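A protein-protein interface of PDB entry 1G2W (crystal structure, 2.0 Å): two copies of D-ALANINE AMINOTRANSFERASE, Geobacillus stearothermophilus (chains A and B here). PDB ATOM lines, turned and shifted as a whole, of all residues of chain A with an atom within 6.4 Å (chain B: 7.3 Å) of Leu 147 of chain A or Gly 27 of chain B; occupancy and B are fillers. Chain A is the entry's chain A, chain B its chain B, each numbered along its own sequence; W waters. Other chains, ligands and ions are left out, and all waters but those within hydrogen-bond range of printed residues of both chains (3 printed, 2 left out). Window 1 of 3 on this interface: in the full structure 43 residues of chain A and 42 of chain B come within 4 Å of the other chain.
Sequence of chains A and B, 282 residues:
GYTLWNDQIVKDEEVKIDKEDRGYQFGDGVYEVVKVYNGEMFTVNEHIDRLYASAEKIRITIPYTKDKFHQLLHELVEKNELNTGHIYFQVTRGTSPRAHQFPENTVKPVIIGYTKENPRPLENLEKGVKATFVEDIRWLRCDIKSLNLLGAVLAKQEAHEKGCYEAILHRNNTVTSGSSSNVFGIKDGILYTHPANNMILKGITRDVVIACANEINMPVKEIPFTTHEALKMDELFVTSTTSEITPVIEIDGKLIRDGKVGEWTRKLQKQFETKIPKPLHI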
ATOM      1  N   GLY A  23     -29.401 -32.792  11.196  1.00  0.00           N
ATOM      2  CA  GLY A  23     -28.497 -31.789  11.712  1.00  0.00           C
ATOM      3  C   GLY A  23     -29.294 -30.534  12.008  1.00  0.00           C
ATOM      4  O   GLY A  23     -28.889 -29.700  12.811  1.00  0.00           O
ATOM      5  N   TYR A  24     -30.452 -30.405  11.361  1.00  0.00           N
ATOM      6  CA  TYR A  24     -31.293 -29.227  11.550  1.00  0.00           C
ATOM      7  C   TYR A  24     -32.302 -29.405  12.679  1.00  0.00           C
ATOM      8  O   TYR A  24     -32.740 -28.433  13.282  1.00  0.00           O
ATOM      9  CB  TYR A  24     -32.037 -28.906  10.245  1.00  0.00           C
ATOM     10  CG  TYR A  24     -32.670 -27.528  10.193  1.00  0.00           C
ATOM     11  CD1 TYR A  24     -31.900 -26.381  10.360  1.00  0.00           C
ATOM     12  CD2 TYR A  24     -34.031 -27.371   9.932  1.00  0.00           C
ATOM     13  CE1 TYR A  24     -32.462 -25.114  10.265  1.00  0.00           C
ATOM     14  CE2 TYR A  24     -34.606 -26.106   9.834  1.00  0.00           C
ATOM     15  CZ  TYR A  24     -33.816 -24.984   9.999  1.00  0.00           C
ATOM     16  OH  TYR A  24     -34.367 -23.732   9.889  1.00  0.00           O
ATOM     17  N   PHE A  26     -31.857 -31.917  15.318  1.00  0.00           N
ATOM     18  CA  PHE A  26     -31.233 -32.424  16.537  1.00  0.00           C
ATOM     19  C   PHE A  26     -29.795 -31.951  16.756  1.00  0.00           C
ATOM     20  O   PHE A  26     -29.226 -32.171  17.831  1.00  0.00           O
ATOM     21  CB  PHE A  26     -31.215 -33.962  16.518  1.00  0.00           C
ATOM     22  CG  PHE A  26     -32.574 -34.593  16.378  1.00  0.00           C
ATOM     23  CD1 PHE A  26     -33.527 -34.463  17.381  1.00  0.00           C
ATOM     24  CD2 PHE A  26     -32.896 -35.325  15.239  1.00  0.00           C
ATOM     25  CE1 PHE A  26     -34.783 -35.051  17.252  1.00  0.00           C
ATOM     26  CE2 PHE A  26     -34.151 -35.919  15.097  1.00  0.00           C
ATOM     27  CZ  PHE A  26     -35.098 -35.781  16.109  1.00  0.00           C
ATOM     28  N   GLY A  27     -29.209 -31.317  15.745  1.00  0.00           N
ATOM     29  CA  GLY A  27     -27.821 -30.907  15.858  1.00  0.00           C
ATOM     30  C   GLY A  27     -27.042 -32.210  15.817  1.00  0.00           C
ATOM     31  O   GLY A  27     -25.941 -32.331  16.362  1.00  0.00           O
ATOM     32  N   ASP A  28     -27.633 -33.193  15.141  1.00  0.00           N
ATOM     33  CA  ASP A  28     -27.062 -34.532  15.027  1.00  0.00           C
ATOM     34  C   ASP A  28     -25.993 -34.622  13.942  1.00  0.00           C
ATOM     35  O   ASP A  28     -26.234 -35.138  12.839  1.00  0.00           O
ATOM     36  CB  ASP A  28     -28.189 -35.536  14.758  1.00  0.00           C
ATOM     37  CG  ASP A  28     -27.733 -36.977  14.856  1.00  0.00           C
ATOM     38  OD1 ASP A  28     -26.585 -37.226  15.292  1.00  0.00           O
ATOM     39  OD2 ASP A  28     -28.535 -37.867  14.503  1.00  0.00           O
ATOM     40  N   GLY A  29     -24.800 -34.132  14.270  1.00  0.00           N
ATOM     41  CA  GLY A  29     -23.710 -34.153  13.320  1.00  0.00           C
ATOM     42  C   GLY A  29     -22.427 -33.637  13.947  1.00  0.00           C
ATOM     43  O   GLY A  29     -22.410 -33.230  15.113  1.00  0.00           O
ATOM     44  N   VAL A  30     -21.354 -33.660  13.168  1.00  0.00           N
ATOM     45  CA  VAL A  30     -20.060 -33.196  13.650  1.00  0.00           C
ATOM     46  C   VAL A  30     -19.426 -32.264  12.622  1.00  0.00           C
ATOM     47  O   VAL A  30     -19.866 -32.212  11.468  1.00  0.00           O
ATOM     48  CB  VAL A  30     -19.139 -34.390  13.949  1.00  0.00           C
ATOM     49  CG1 VAL A  30     -19.791 -35.275  15.023  1.00  0.00           C
ATOM     50  CG2 VAL A  30     -18.861 -35.187  12.666  1.00  0.00           C
ATOM     51  N   TYR A  31     -18.401 -31.524  13.038  1.00  0.00           N
ATOM     52  CA  TYR A  31     -17.754 -30.573  12.140  1.00  0.00           C
ATOM     53  C   TYR A  31     -16.279 -30.341  12.468  1.00  0.00           C
ATOM     54  O   TYR A  31     -15.792 -30.738  13.527  1.00  0.00           O
ATOM     55  CB  TYR A  31     -18.481 -29.226  12.198  1.00  0.00           C
ATOM     56  CG  TYR A  31     -18.162 -28.420  13.447  1.00  0.00           C
ATOM     57  CD1 TYR A  31     -18.716 -28.757  14.681  1.00  0.00           C
ATOM     58  CD2 TYR A  31     -17.268 -27.350  13.395  1.00  0.00           C
ATOM     59  CE1 TYR A  31     -18.388 -28.053  15.837  1.00  0.00           C
ATOM     60  CE2 TYR A  31     -16.931 -26.637  14.541  1.00  0.00           C
ATOM     61  CZ  TYR A  31     -17.494 -26.994  15.757  1.00  0.00           C
ATOM     62  OH  TYR A  31     -17.164 -26.298  16.894  1.00  0.00           O
ATOM     63  N   TYR A  88     -14.654 -24.822   6.327  1.00  0.00           N
ATOM     64  CA  TYR A  88     -15.584 -25.353   7.312  1.00  0.00           C
ATOM     65  C   TYR A  88     -16.295 -26.538   6.672  1.00  0.00           C
ATOM     66  O   TYR A  88     -16.788 -26.430   5.546  1.00  0.00           O
ATOM     67  CB  TYR A  88     -16.639 -24.313   7.707  1.00  0.00           C
ATOM     68  CG  TYR A  88     -17.734 -24.897   8.577  1.00  0.00           C
ATOM     69  CD1 TYR A  88     -17.579 -24.983   9.961  1.00  0.00           C
ATOM     70  CD2 TYR A  88     -18.897 -25.429   8.012  1.00  0.00           C
ATOM     71  CE1 TYR A  88     -18.546 -25.585  10.761  1.00  0.00           C
ATOM     72  CE2 TYR A  88     -19.876 -26.041   8.803  1.00  0.00           C
ATOM     73  CZ  TYR A  88     -19.693 -26.116  10.178  1.00  0.00           C
ATOM     74  OH  TYR A  88     -20.639 -26.726  10.968  1.00  0.00           O
ATOM     75  N   GLN A  90     -18.893 -30.117   7.689  1.00  0.00           N
ATOM     76  CA  GLN A  90     -19.652 -30.859   8.679  1.00  0.00           C
ATOM     77  C   GLN A  90     -20.372 -32.036   8.035  1.00  0.00           C
ATOM     78  O   GLN A  90     -20.610 -32.052   6.816  1.00  0.00           O
ATOM     79  CB  GLN A  90     -20.681 -29.937   9.345  1.00  0.00           C
ATOM     80  CG  GLN A  90     -21.726 -29.404   8.366  1.00  0.00           C
ATOM     81  CD  GLN A  90     -22.847 -28.650   9.050  1.00  0.00           C
ATOM     82  OE1 GLN A  90     -22.647 -27.557   9.584  1.00  0.00           O
ATOM     83  NE2 GLN A  90     -24.039 -29.234   9.040  1.00  0.00           N
ATOM     84  N   VAL A  91     -20.716 -33.015   8.865  1.00  0.00           N
ATOM     85  CA  VAL A  91     -21.434 -34.204   8.426  1.00  0.00           C
ATOM     86  C   VAL A  91     -22.595 -34.440   9.388  1.00  0.00           C
ATOM     87  O   VAL A  91     -22.389 -34.452  10.606  1.00  0.00           O
ATOM     88  CB  VAL A  91     -20.522 -35.453   8.466  1.00  0.00           C
ATOM     89  CG1 VAL A  91     -21.277 -36.675   7.939  1.00  0.00           C
ATOM     90  CG2 VAL A  91     -19.266 -35.203   7.651  1.00  0.00           C
ATOM     91  N   THR A  92     -23.812 -34.604   8.867  1.00  0.00           N
ATOM     92  CA  THR A  92     -24.951 -34.880   9.740  1.00  0.00           C
ATOM     93  C   THR A  92     -25.414 -36.298   9.426  1.00  0.00           C
ATOM     94  O   THR A  92     -25.067 -36.848   8.375  1.00  0.00           O
ATOM     95  CB  THR A  92     -26.134 -33.923   9.508  1.00  0.00           C
ATOM     96  OG1 THR A  92     -26.817 -34.293   8.304  1.00  0.00           O
ATOM     97  CG2 THR A  92     -25.650 -32.486   9.414  1.00  0.00           C
ATOM     98  N   LYS A 145     -16.648 -33.156  18.673  1.00  0.00           N
ATOM     99  CA  LYS A 145     -16.811 -31.825  18.092  1.00  0.00           C
ATOM    100  C   LYS A 145     -18.151 -31.857  17.325  1.00  0.00           C
ATOM    101  O   LYS A 145     -18.179 -31.986  16.096  1.00  0.00           O
ATOM    102  CB  LYS A 145     -15.639 -31.498  17.150  1.00  0.00           C
ATOM    103  CG  LYS A 145     -15.383 -29.994  17.008  1.00  0.00           C
ATOM    104  CD  LYS A 145     -14.177 -29.673  16.118  1.00  0.00           C
ATOM    105  CE  LYS A 145     -13.881 -28.178  16.106  1.00  0.00           C
ATOM    106  NZ  LYS A 145     -13.754 -27.709  17.479  1.00  0.00           N
ATOM    107  N   SER A 146     -19.252 -31.744  18.066  1.00  0.00           N
ATOM    108  CA  SER A 146     -20.592 -31.806  17.472  1.00  0.00           C
ATOM    109  C   SER A 146     -21.264 -30.458  17.244  1.00  0.00           C
ATOM    110  O   SER A 146     -20.790 -29.413  17.717  1.00  0.00           O
ATOM    111  CB  SER A 146     -21.510 -32.660  18.352  1.00  0.00           C
ATOM    112  OG  SER A 146     -21.982 -31.899  19.450  1.00  0.00           O
ATOM    113  N   LEU A 147     -22.392 -30.510  16.535  1.00  0.00           N
ATOM    114  CA  LEU A 147     -23.184 -29.330  16.201  1.00  0.00           C
ATOM    115  C   LEU A 147     -24.032 -28.799  17.361  1.00  0.00           C
ATOM    116  O   LEU A 147     -24.695 -27.775  17.216  1.00  0.00           O
ATOM    117  CB  LEU A 147     -24.084 -29.628  14.984  1.00  0.00           C
ATOM    118  CG  LEU A 147     -23.356 -29.916  13.662  1.00  0.00           C
ATOM    119  CD1 LEU A 147     -24.354 -30.422  12.617  1.00  0.00           C
ATOM    120  CD2 LEU A 147     -22.659 -28.652  13.157  1.00  0.00           C
ATOM    121  N   ASN A 148     -24.021 -29.492  18.499  1.00  0.00           N
ATOM    122  CA  ASN A 148     -24.774 -29.040  19.678  1.00  0.00           C
ATOM    123  C   ASN A 148     -23.904 -27.966  20.337  1.00  0.00           C
ATOM    124  O   ASN A 148     -23.175 -28.243  21.293  1.00  0.00           O
ATOM    125  CB  ASN A 148     -25.002 -30.191  20.667  1.00  0.00           C
ATOM    126  CG  ASN A 148     -26.229 -31.027  20.332  1.00  0.00           C
ATOM    127  OD1 ASN A 148     -26.914 -31.519  21.234  1.00  0.00           O
ATOM    128  ND2 ASN A 148     -26.507 -31.206  19.043  1.00  0.00           N
ATOM    129  N   LEU A 149     -24.003 -26.739  19.832  1.00  0.00           N
ATOM    130  CA  LEU A 149     -23.179 -25.636  20.309  1.00  0.00           C
ATOM    131  C   LEU A 149     -23.904 -24.498  21.009  1.00  0.00           C
ATOM    132  O   LEU A 149     -23.368 -23.386  21.114  1.00  0.00           O
ATOM    133  CB  LEU A 149     -22.392 -25.078  19.122  1.00  0.00           C
ATOM    134  CG  LEU A 149     -21.406 -26.080  18.518  1.00  0.00           C
ATOM    135  CD1 LEU A 149     -20.945 -25.641  17.125  1.00  0.00           C
ATOM    136  CD2 LEU A 149     -20.227 -26.211  19.474  1.00  0.00           C
ATOM    137  N   LEU A 150     -25.110 -24.761  21.497  1.00  0.00           N
ATOM    138  CA  LEU A 150     -25.880 -23.721  22.161  1.00  0.00           C
ATOM    139  C   LEU A 150     -25.178 -23.220  23.423  1.00  0.00           C
ATOM    140  O   LEU A 150     -25.281 -22.044  23.770  1.00  0.00           O
ATOM    141  CB  LEU A 150     -27.282 -24.234  22.485  1.00  0.00           C
ATOM    142  CG  LEU A 150     -28.331 -23.182  22.854  1.00  0.00           C
ATOM    143  CD1 LEU A 150     -28.273 -21.983  21.902  1.00  0.00           C
ATOM    144  CD2 LEU A 150     -29.708 -23.849  22.813  1.00  0.00           C
ATOM    145  N   ASP B  21     -27.926 -21.468   8.374  1.00  0.00           N
ATOM    146  CA  ASP B  21     -29.054 -21.224   9.259  1.00  0.00           C
ATOM    147  C   ASP B  21     -28.420 -21.653  10.583  1.00  0.00           C
ATOM    148  O   ASP B  21     -27.842 -22.744  10.661  1.00  0.00           O
ATOM    149  CB  ASP B  21     -30.223 -22.155   8.914  1.00  0.00           C
ATOM    150  CG  ASP B  21     -31.434 -21.934   9.809  1.00  0.00           C
ATOM    151  OD1 ASP B  21     -31.261 -21.908  11.050  1.00  0.00           O
ATOM    152  OD2 ASP B  21     -32.563 -21.792   9.273  1.00  0.00           O
ATOM    153  N   ARG B  22     -28.510 -20.814  11.610  1.00  0.00           N
ATOM    154  CA  ARG B  22     -27.897 -21.152  12.886  1.00  0.00           C
ATOM    155  C   ARG B  22     -28.472 -22.412  13.532  1.00  0.00           C
ATOM    156  O   ARG B  22     -27.855 -23.001  14.424  1.00  0.00           O
ATOM    157  CB  ARG B  22     -27.967 -19.948  13.832  1.00  0.00           C
ATOM    158  CG  ARG B  22     -27.045 -18.803  13.379  1.00  0.00           C
ATOM    159  CD  ARG B  22     -27.275 -17.524  14.173  1.00  0.00           C
ATOM    160  NE  ARG B  22     -26.901 -17.678  15.573  1.00  0.00           N
ATOM    161  CZ  ARG B  22     -25.670 -17.511  16.047  1.00  0.00           C
ATOM    162  NH1 ARG B  22     -24.674 -17.180  15.235  1.00  0.00           N
ATOM    163  NH2 ARG B  22     -25.436 -17.678  17.340  1.00  0.00           N
ATOM    164  N   GLY B  23     -29.649 -22.834  13.075  1.00  0.00           N
ATOM    165  CA  GLY B  23     -30.233 -24.051  13.610  1.00  0.00           C
ATOM    166  C   GLY B  23     -29.477 -25.259  13.074  1.00  0.00           C
ATOM    167  O   GLY B  23     -29.404 -26.315  13.712  1.00  0.00           O
ATOM    168  N   TYR B  24     -28.891 -25.094  11.895  1.00  0.00           N
ATOM    169  CA  TYR B  24     -28.153 -26.169  11.245  1.00  0.00           C
ATOM    170  C   TYR B  24     -26.681 -26.238  11.644  1.00  0.00           C
ATOM    171  O   TYR B  24     -26.054 -27.286  11.505  1.00  0.00           O
ATOM    172  CB  TYR B  24     -28.250 -26.001   9.730  1.00  0.00           C
ATOM    173  CG  TYR B  24     -27.810 -27.202   8.919  1.00  0.00           C
ATOM    174  CD1 TYR B  24     -28.330 -28.464   9.172  1.00  0.00           C
ATOM    175  CD2 TYR B  24     -26.933 -27.059   7.844  1.00  0.00           C
ATOM    176  CE1 TYR B  24     -27.991 -29.557   8.372  1.00  0.00           C
ATOM    177  CE2 TYR B  24     -26.590 -28.146   7.037  1.00  0.00           C
ATOM    178  CZ  TYR B  24     -27.127 -29.387   7.306  1.00  0.00           C
ATOM    179  OH  TYR B  24     -26.812 -30.461   6.504  1.00  0.00           O
ATOM    180  N   GLN B  25     -26.121 -25.133  12.132  1.00  0.00           N
ATOM    181  CA  GLN B  25     -24.706 -25.138  12.512  1.00  0.00           C
ATOM    182  C   GLN B  25     -24.456 -25.148  14.020  1.00  0.00           C
ATOM    183  O   GLN B  25     -23.403 -25.601  14.469  1.00  0.00           O
ATOM    184  CB  GLN B  25     -23.974 -23.947  11.871  1.00  0.00           C
ATOM    185  CG  GLN B  25     -23.996 -23.953  10.337  1.00  0.00           C
ATOM    186  CD  GLN B  25     -23.072 -22.910   9.718  1.00  0.00           C
ATOM    187  OE1 GLN B  25     -23.095 -21.732  10.095  1.00  0.00           O
ATOM    188  NE2 GLN B  25     -22.266 -23.336   8.755  1.00  0.00           N
ATOM    189  N   PHE B  26     -25.426 -24.671  14.796  1.00  0.00           N
ATOM    190  CA  PHE B  26     -25.298 -24.613  16.254  1.00  0.00           C
ATOM    191  C   PHE B  26     -26.476 -25.236  17.002  1.00  0.00           C
ATOM    192  O   PHE B  26     -26.456 -25.322  18.236  1.00  0.00           O
ATOM    193  CB  PHE B  26     -25.177 -23.156  16.710  1.00  0.00           C
ATOM    194  CG  PHE B  26     -24.080 -22.388  16.031  1.00  0.00           C
ATOM    195  CD1 PHE B  26     -22.743 -22.652  16.316  1.00  0.00           C
ATOM    196  CD2 PHE B  26     -24.383 -21.396  15.107  1.00  0.00           C
ATOM    197  CE1 PHE B  26     -21.716 -21.929  15.682  1.00  0.00           C
ATOM    198  CE2 PHE B  26     -23.374 -20.671  14.468  1.00  0.00           C
ATOM    199  CZ  PHE B  26     -22.039 -20.938  14.757  1.00  0.00           C
ATOM    200  N   GLY B  27     -27.504 -25.667  16.276  1.00  0.00           N
ATOM    201  CA  GLY B  27     -28.677 -26.206  16.945  1.00  0.00           C
ATOM    202  C   GLY B  27     -29.261 -25.052  17.747  1.00  0.00           C
ATOM    203  O   GLY B  27     -29.926 -25.248  18.760  1.00  0.00           O
ATOM    204  N   ASP B  28     -29.002 -23.837  17.267  1.00  0.00           N
ATOM    205  CA  ASP B  28     -29.436 -22.590  17.909  1.00  0.00           C
ATOM    206  C   ASP B  28     -30.910 -22.242  17.629  1.00  0.00           C
ATOM    207  O   ASP B  28     -31.224 -21.365  16.818  1.00  0.00           O
ATOM    208  CB  ASP B  28     -28.494 -21.464  17.440  1.00  0.00           C
ATOM    209  CG  ASP B  28     -28.747 -20.123  18.124  1.00  0.00           C
ATOM    210  OD1 ASP B  28     -29.425 -20.067  19.174  1.00  0.00           O
ATOM    211  OD2 ASP B  28     -28.233 -19.109  17.598  1.00  0.00           O
ATOM    212  N   GLY B  29     -31.811 -22.937  18.319  1.00  0.00           N
ATOM    213  CA  GLY B  29     -33.230 -22.697  18.136  1.00  0.00           C
ATOM    214  C   GLY B  29     -34.060 -23.478  19.137  1.00  0.00           C
ATOM    215  O   GLY B  29     -33.521 -24.270  19.908  1.00  0.00           O
ATOM    216  N   VAL B  30     -35.373 -23.266  19.120  1.00  0.00           N
ATOM    217  CA  VAL B  30     -36.269 -23.954  20.044  1.00  0.00           C
ATOM    218  C   VAL B  30     -37.444 -24.580  19.288  1.00  0.00           C
ATOM    219  O   VAL B  30     -37.711 -24.208  18.137  1.00  0.00           O
ATOM    220  CB  VAL B  30     -36.797 -22.982  21.122  1.00  0.00           C
ATOM    221  CG1 VAL B  30     -35.619 -22.458  21.971  1.00  0.00           C
ATOM    222  CG2 VAL B  30     -37.530 -21.821  20.470  1.00  0.00           C
ATOM    223  N   ILE B  58     -33.147 -17.993  25.429  1.00  0.00           N
ATOM    224  CA  ILE B  58     -31.911 -17.925  24.643  1.00  0.00           C
ATOM    225  C   ILE B  58     -31.902 -16.657  23.796  1.00  0.00           C
ATOM    226  O   ILE B  58     -31.157 -16.537  22.823  1.00  0.00           O
ATOM    227  CB  ILE B  58     -31.661 -19.188  23.738  1.00  0.00           C
ATOM    228  CG1 ILE B  58     -32.727 -19.323  22.644  1.00  0.00           C
ATOM    229  CG2 ILE B  58     -31.612 -20.439  24.600  1.00  0.00           C
ATOM    230  CD1 ILE B  58     -32.454 -20.494  21.687  1.00  0.00           C
ATOM    231  N   VAL B  91     -38.140 -22.636  15.809  1.00  0.00           N
ATOM    232  CA  VAL B  91     -37.676 -21.287  15.520  1.00  0.00           C
ATOM    233  C   VAL B  91     -36.165 -21.259  15.764  1.00  0.00           C
ATOM    234  O   VAL B  91     -35.699 -21.650  16.839  1.00  0.00           O
ATOM    235  CB  VAL B  91     -38.323 -20.256  16.472  1.00  0.00           C
ATOM    236  CG1 VAL B  91     -37.929 -18.844  16.057  1.00  0.00           C
ATOM    237  CG2 VAL B  91     -39.832 -20.422  16.487  1.00  0.00           C
ATOM    238  N   THR B  92     -35.403 -20.827  14.766  1.00  0.00           N
ATOM    239  CA  THR B  92     -33.954 -20.727  14.909  1.00  0.00           C
ATOM    240  C   THR B  92     -33.622 -19.240  14.892  1.00  0.00           C
ATOM    241  O   THR B  92     -34.434 -18.424  14.433  1.00  0.00           O
ATOM    242  CB  THR B  92     -33.198 -21.437  13.763  1.00  0.00           C
ATOM    243  OG1 THR B  92     -33.322 -20.677  12.556  1.00  0.00           O
ATOM    244  CG2 THR B  92     -33.758 -22.842  13.536  1.00  0.00           C
ATOM    245  N   ARG B  98     -21.353 -17.816   9.637  1.00  0.00           N
ATOM    246  CA  ARG B  98     -20.972 -18.540  10.844  1.00  0.00           C
ATOM    247  C   ARG B  98     -20.113 -17.791  11.850  1.00  0.00           C
ATOM    248  O   ARG B  98     -19.002 -17.350  11.544  1.00  0.00           O
ATOM    249  CB  ARG B  98     -20.271 -19.852  10.494  1.00  0.00           C
ATOM    250  CG  ARG B  98     -19.990 -20.708  11.724  1.00  0.00           C
ATOM    251  CD  ARG B  98     -19.431 -22.072  11.368  1.00  0.00           C
ATOM    252  NE  ARG B  98     -19.434 -22.971  12.521  1.00  0.00           N
ATOM    253  CZ  ARG B  98     -18.505 -22.985  13.474  1.00  0.00           C
ATOM    254  NH1 ARG B  98     -17.476 -22.143  13.419  1.00  0.00           N
ATOM    255  NH2 ARG B  98     -18.603 -23.838  14.484  1.00  0.00           N
ATOM    256  N   SER B 146     -34.755 -26.912  23.490  1.00  0.00           N
ATOM    257  CA  SER B 146     -33.913 -26.533  22.353  1.00  0.00           C
ATOM    258  C   SER B 146     -33.606 -27.653  21.369  1.00  0.00           C
ATOM    259  O   SER B 146     -33.888 -28.828  21.617  1.00  0.00           O
ATOM    260  CB  SER B 146     -32.576 -25.972  22.847  1.00  0.00           C
ATOM    261  OG  SER B 146     -31.718 -27.039  23.216  1.00  0.00           O
ATOM    262  N   LEU B 147     -32.993 -27.262  20.256  1.00  0.00           N
ATOM    263  CA  LEU B 147     -32.614 -28.185  19.198  1.00  0.00           C
ATOM    264  C   LEU B 147     -31.332 -28.955  19.504  1.00  0.00           C
ATOM    265  O   LEU B 147     -30.926 -29.818  18.722  1.00  0.00           O
ATOM    266  CB  LEU B 147     -32.458 -27.427  17.875  1.00  0.00           C
ATOM    267  CG  LEU B 147     -33.708 -26.686  17.386  1.00  0.00           C
ATOM    268  CD1 LEU B 147     -33.396 -26.002  16.064  1.00  0.00           C
ATOM    269  CD2 LEU B 147     -34.874 -27.665  17.224  1.00  0.00           C
ATOM    270  N   ASN B 148     -30.674 -28.633  20.617  1.00  0.00           N
ATOM    271  CA  ASN B 148     -29.458 -29.366  20.990  1.00  0.00           C
ATOM    272  C   ASN B 148     -29.981 -30.657  21.612  1.00  0.00           C
ATOM    273  O   ASN B 148     -30.165 -30.739  22.827  1.00  0.00           O
ATOM    274  CB  ASN B 148     -28.628 -28.588  22.023  1.00  0.00           C
ATOM    275  CG  ASN B 148     -27.664 -27.606  21.381  1.00  0.00           C
ATOM    276  OD1 ASN B 148     -26.536 -27.436  21.848  1.00  0.00           O
ATOM    277  ND2 ASN B 148     -28.103 -26.951  20.310  1.00  0.00           N
ATOM    278  N   LEU B 149     -30.212 -31.664  20.774  1.00  0.00           N
ATOM    279  CA  LEU B 149     -30.789 -32.925  21.235  1.00  0.00           C
ATOM    280  C   LEU B 149     -29.933 -34.172  21.091  1.00  0.00           C
ATOM    281  O   LEU B 149     -30.440 -35.294  21.192  1.00  0.00           O
ATOM    282  CB  LEU B 149     -32.118 -33.147  20.505  1.00  0.00           C
ATOM    283  CG  LEU B 149     -33.258 -32.207  20.902  1.00  0.00           C
ATOM    284  CD1 LEU B 149     -34.391 -32.288  19.868  1.00  0.00           C
ATOM    285  CD2 LEU B 149     -33.755 -32.584  22.307  1.00  0.00           C
ATOM    286  N   LEU B 150     -28.638 -33.987  20.871  1.00  0.00           N
ATOM    287  CA  LEU B 150     -27.745 -35.130  20.694  1.00  0.00           C
ATOM    288  C   LEU B 150     -27.755 -36.082  21.898  1.00  0.00           C
ATOM    289  O   LEU B 150     -27.604 -37.293  21.739  1.00  0.00           O
ATOM    290  CB  LEU B 150     -26.325 -34.631  20.388  1.00  0.00           C
ATOM    291  CG  LEU B 150     -25.370 -35.612  19.706  1.00  0.00           C
ATOM    292  CD1 LEU B 150     -26.104 -36.423  18.641  1.00  0.00           C
ATOM    293  CD2 LEU B 150     -24.213 -34.836  19.084  1.00  0.00           C
HETATM  294  O   HOH W   1     -20.944 -25.167  13.226  1.00  0.00           O
HETATM  295  O   HOH W   2     -24.262 -31.324   6.577  1.00  0.00           O
HETATM  296  O   HOH W   3     -23.371 -25.671   7.269  1.00  0.00           O
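CE2 of Tyr 88 of chain A touches NE2 of Gln 25 of chain B (3.6 Å). OE1 of Gln 90 of chain A touches CG of Gln 25 of chain B, 3.9 Å away. C of Asn 148 of chain A touches OD1 of Asn 148 of chain B (3.1 Å). CD1 of Leu 149 of chain A touches O of Gln 25 of chain B, 3.6 Å away. Phe 26 of chain B touches Leu 150 of chain A (O to N, 3.6 Å). Leu 150 of chain A touches Ser 146 of chain B.
Tyr 24 of chain A touches Thr 92 of chain B, and with the chains exchanged Thr 92 of chain A touches Tyr 24 of chain B. Gly 27 of chain A touches Leu 147 of chain B, and with the chains exchanged Leu 147 of chain A touches Gly 27 of chain B. Positions printed for both chains: 23, 24, 26, 27, 28, 29, 30, 91, 92, 146, 147, 148, 149 and 150.
Hydrophobic or aromatic side chains of chain B within 4 Å of the printed part of chain A: Tyr 24, Phe 26, Leu 147, Leu 149 and Leu 150. Along chain B the printed residues that touch a printed residue of chain A span positions 21 to 150. Among the printed residues, no Asp or Glu carboxylate lies within 4 Å of a Lys or Arg side-chain nitrogen of the other chain.
The backbone NH (N) of Gly 27 of chain B lies within hydrogen-bond range of the backbone carbonyl oxygen (O) of Arg 22 of chain B (3.3 Å). O of Phe 26 of chain B lies within hydrogen-bond range of ND2 of Asn 148 of chain B (3.1 Å). The backbone carbonyl oxygen of Gly 27 of chain B lies within hydrogen-bond range of the side-chain amide nitrogen of Asn 148 of chain B.
Water W2 bridges OH of Tyr 24 of chain B (2.7 Å) and NE2 of Gln 90 of chain A (3.2 Å). Water W1 lies within hydrogen-bond range of NE of Arg 98 of chain B (2.8 Å), OH of Tyr 88 of chain A (2.8 Å) and O of Gln 25 of chain B (2.8 Å). Water W3 lies within hydrogen-bond range of NE2 of Gln 25 of chain B (3.0 Å) and OE1 of Gln 90 of chain A (3.1 Å).
Of the printed residues of chain B, Tyr 88 of chain A touches Gln 25 (3.6 Å) and Arg 98 (3.3 Å). Leu 147 of chain A touches four residues of chain B. Printed residues of chain A within 4 Å of Tyr 24 of chain B: Gly 23 (3.6 Å), Tyr 24 (3.6 Å), Gln 90 (3.4 Å), Thr 92 (3.7 Å) and Leu 147 (3.7 Å). Gly 27 of chain B touches just one residue of chain A: Leu 147. Gly 29 of chain B touches none of the printed residues of chain A. The nearest printed residue of chain A that does not touch Asp 21 of chain B is Gln 90 of chain A (7.2 Å).
The side-chain carboxylate (OD2) of Asp 21 of chain B is in hydrogen-bond range of the side-chain hydroxyl (OH) of Tyr 24 of chain A, at 2.7 Å. The backbone carbonyl oxygen (O) of Phe 26 of chain A lies within hydrogen-bond range of the backbone NH (N) of Leu 149 of chain B (3.1 Å). The backbone NH of Leu 149 of chain B lies within hydrogen-bond range of the side-chain amide oxygen of Asn 148 of chain A, 3.3 Å away. The backbone NH (N) of Leu 150 of chain B lies within hydrogen-bond range of the side-chain amide oxygen (OD1) of Asn 148 of chain A (3.0 Å). O of Phe 26 of chain B lies within hydrogen-bond range of N of Leu 149 of chain A. The side-chain amide oxygen (OD1) of Asn 148 of chain B sits at hydrogen-bond distance from the backbone NH (N) of Leu 149 of chain A. The backbone NH of Leu 150 of chain A lies within hydrogen-bond range of the side-chain amide oxygen of Asn 148 of chain B (3.1 Å). O of Phe 26 of chain A lies close to O of Leu 147 of chain B, at 3.0 Å. O of Phe 26 of chain B lies close to O of Leu 147 of chain A, 3.2 Å away.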
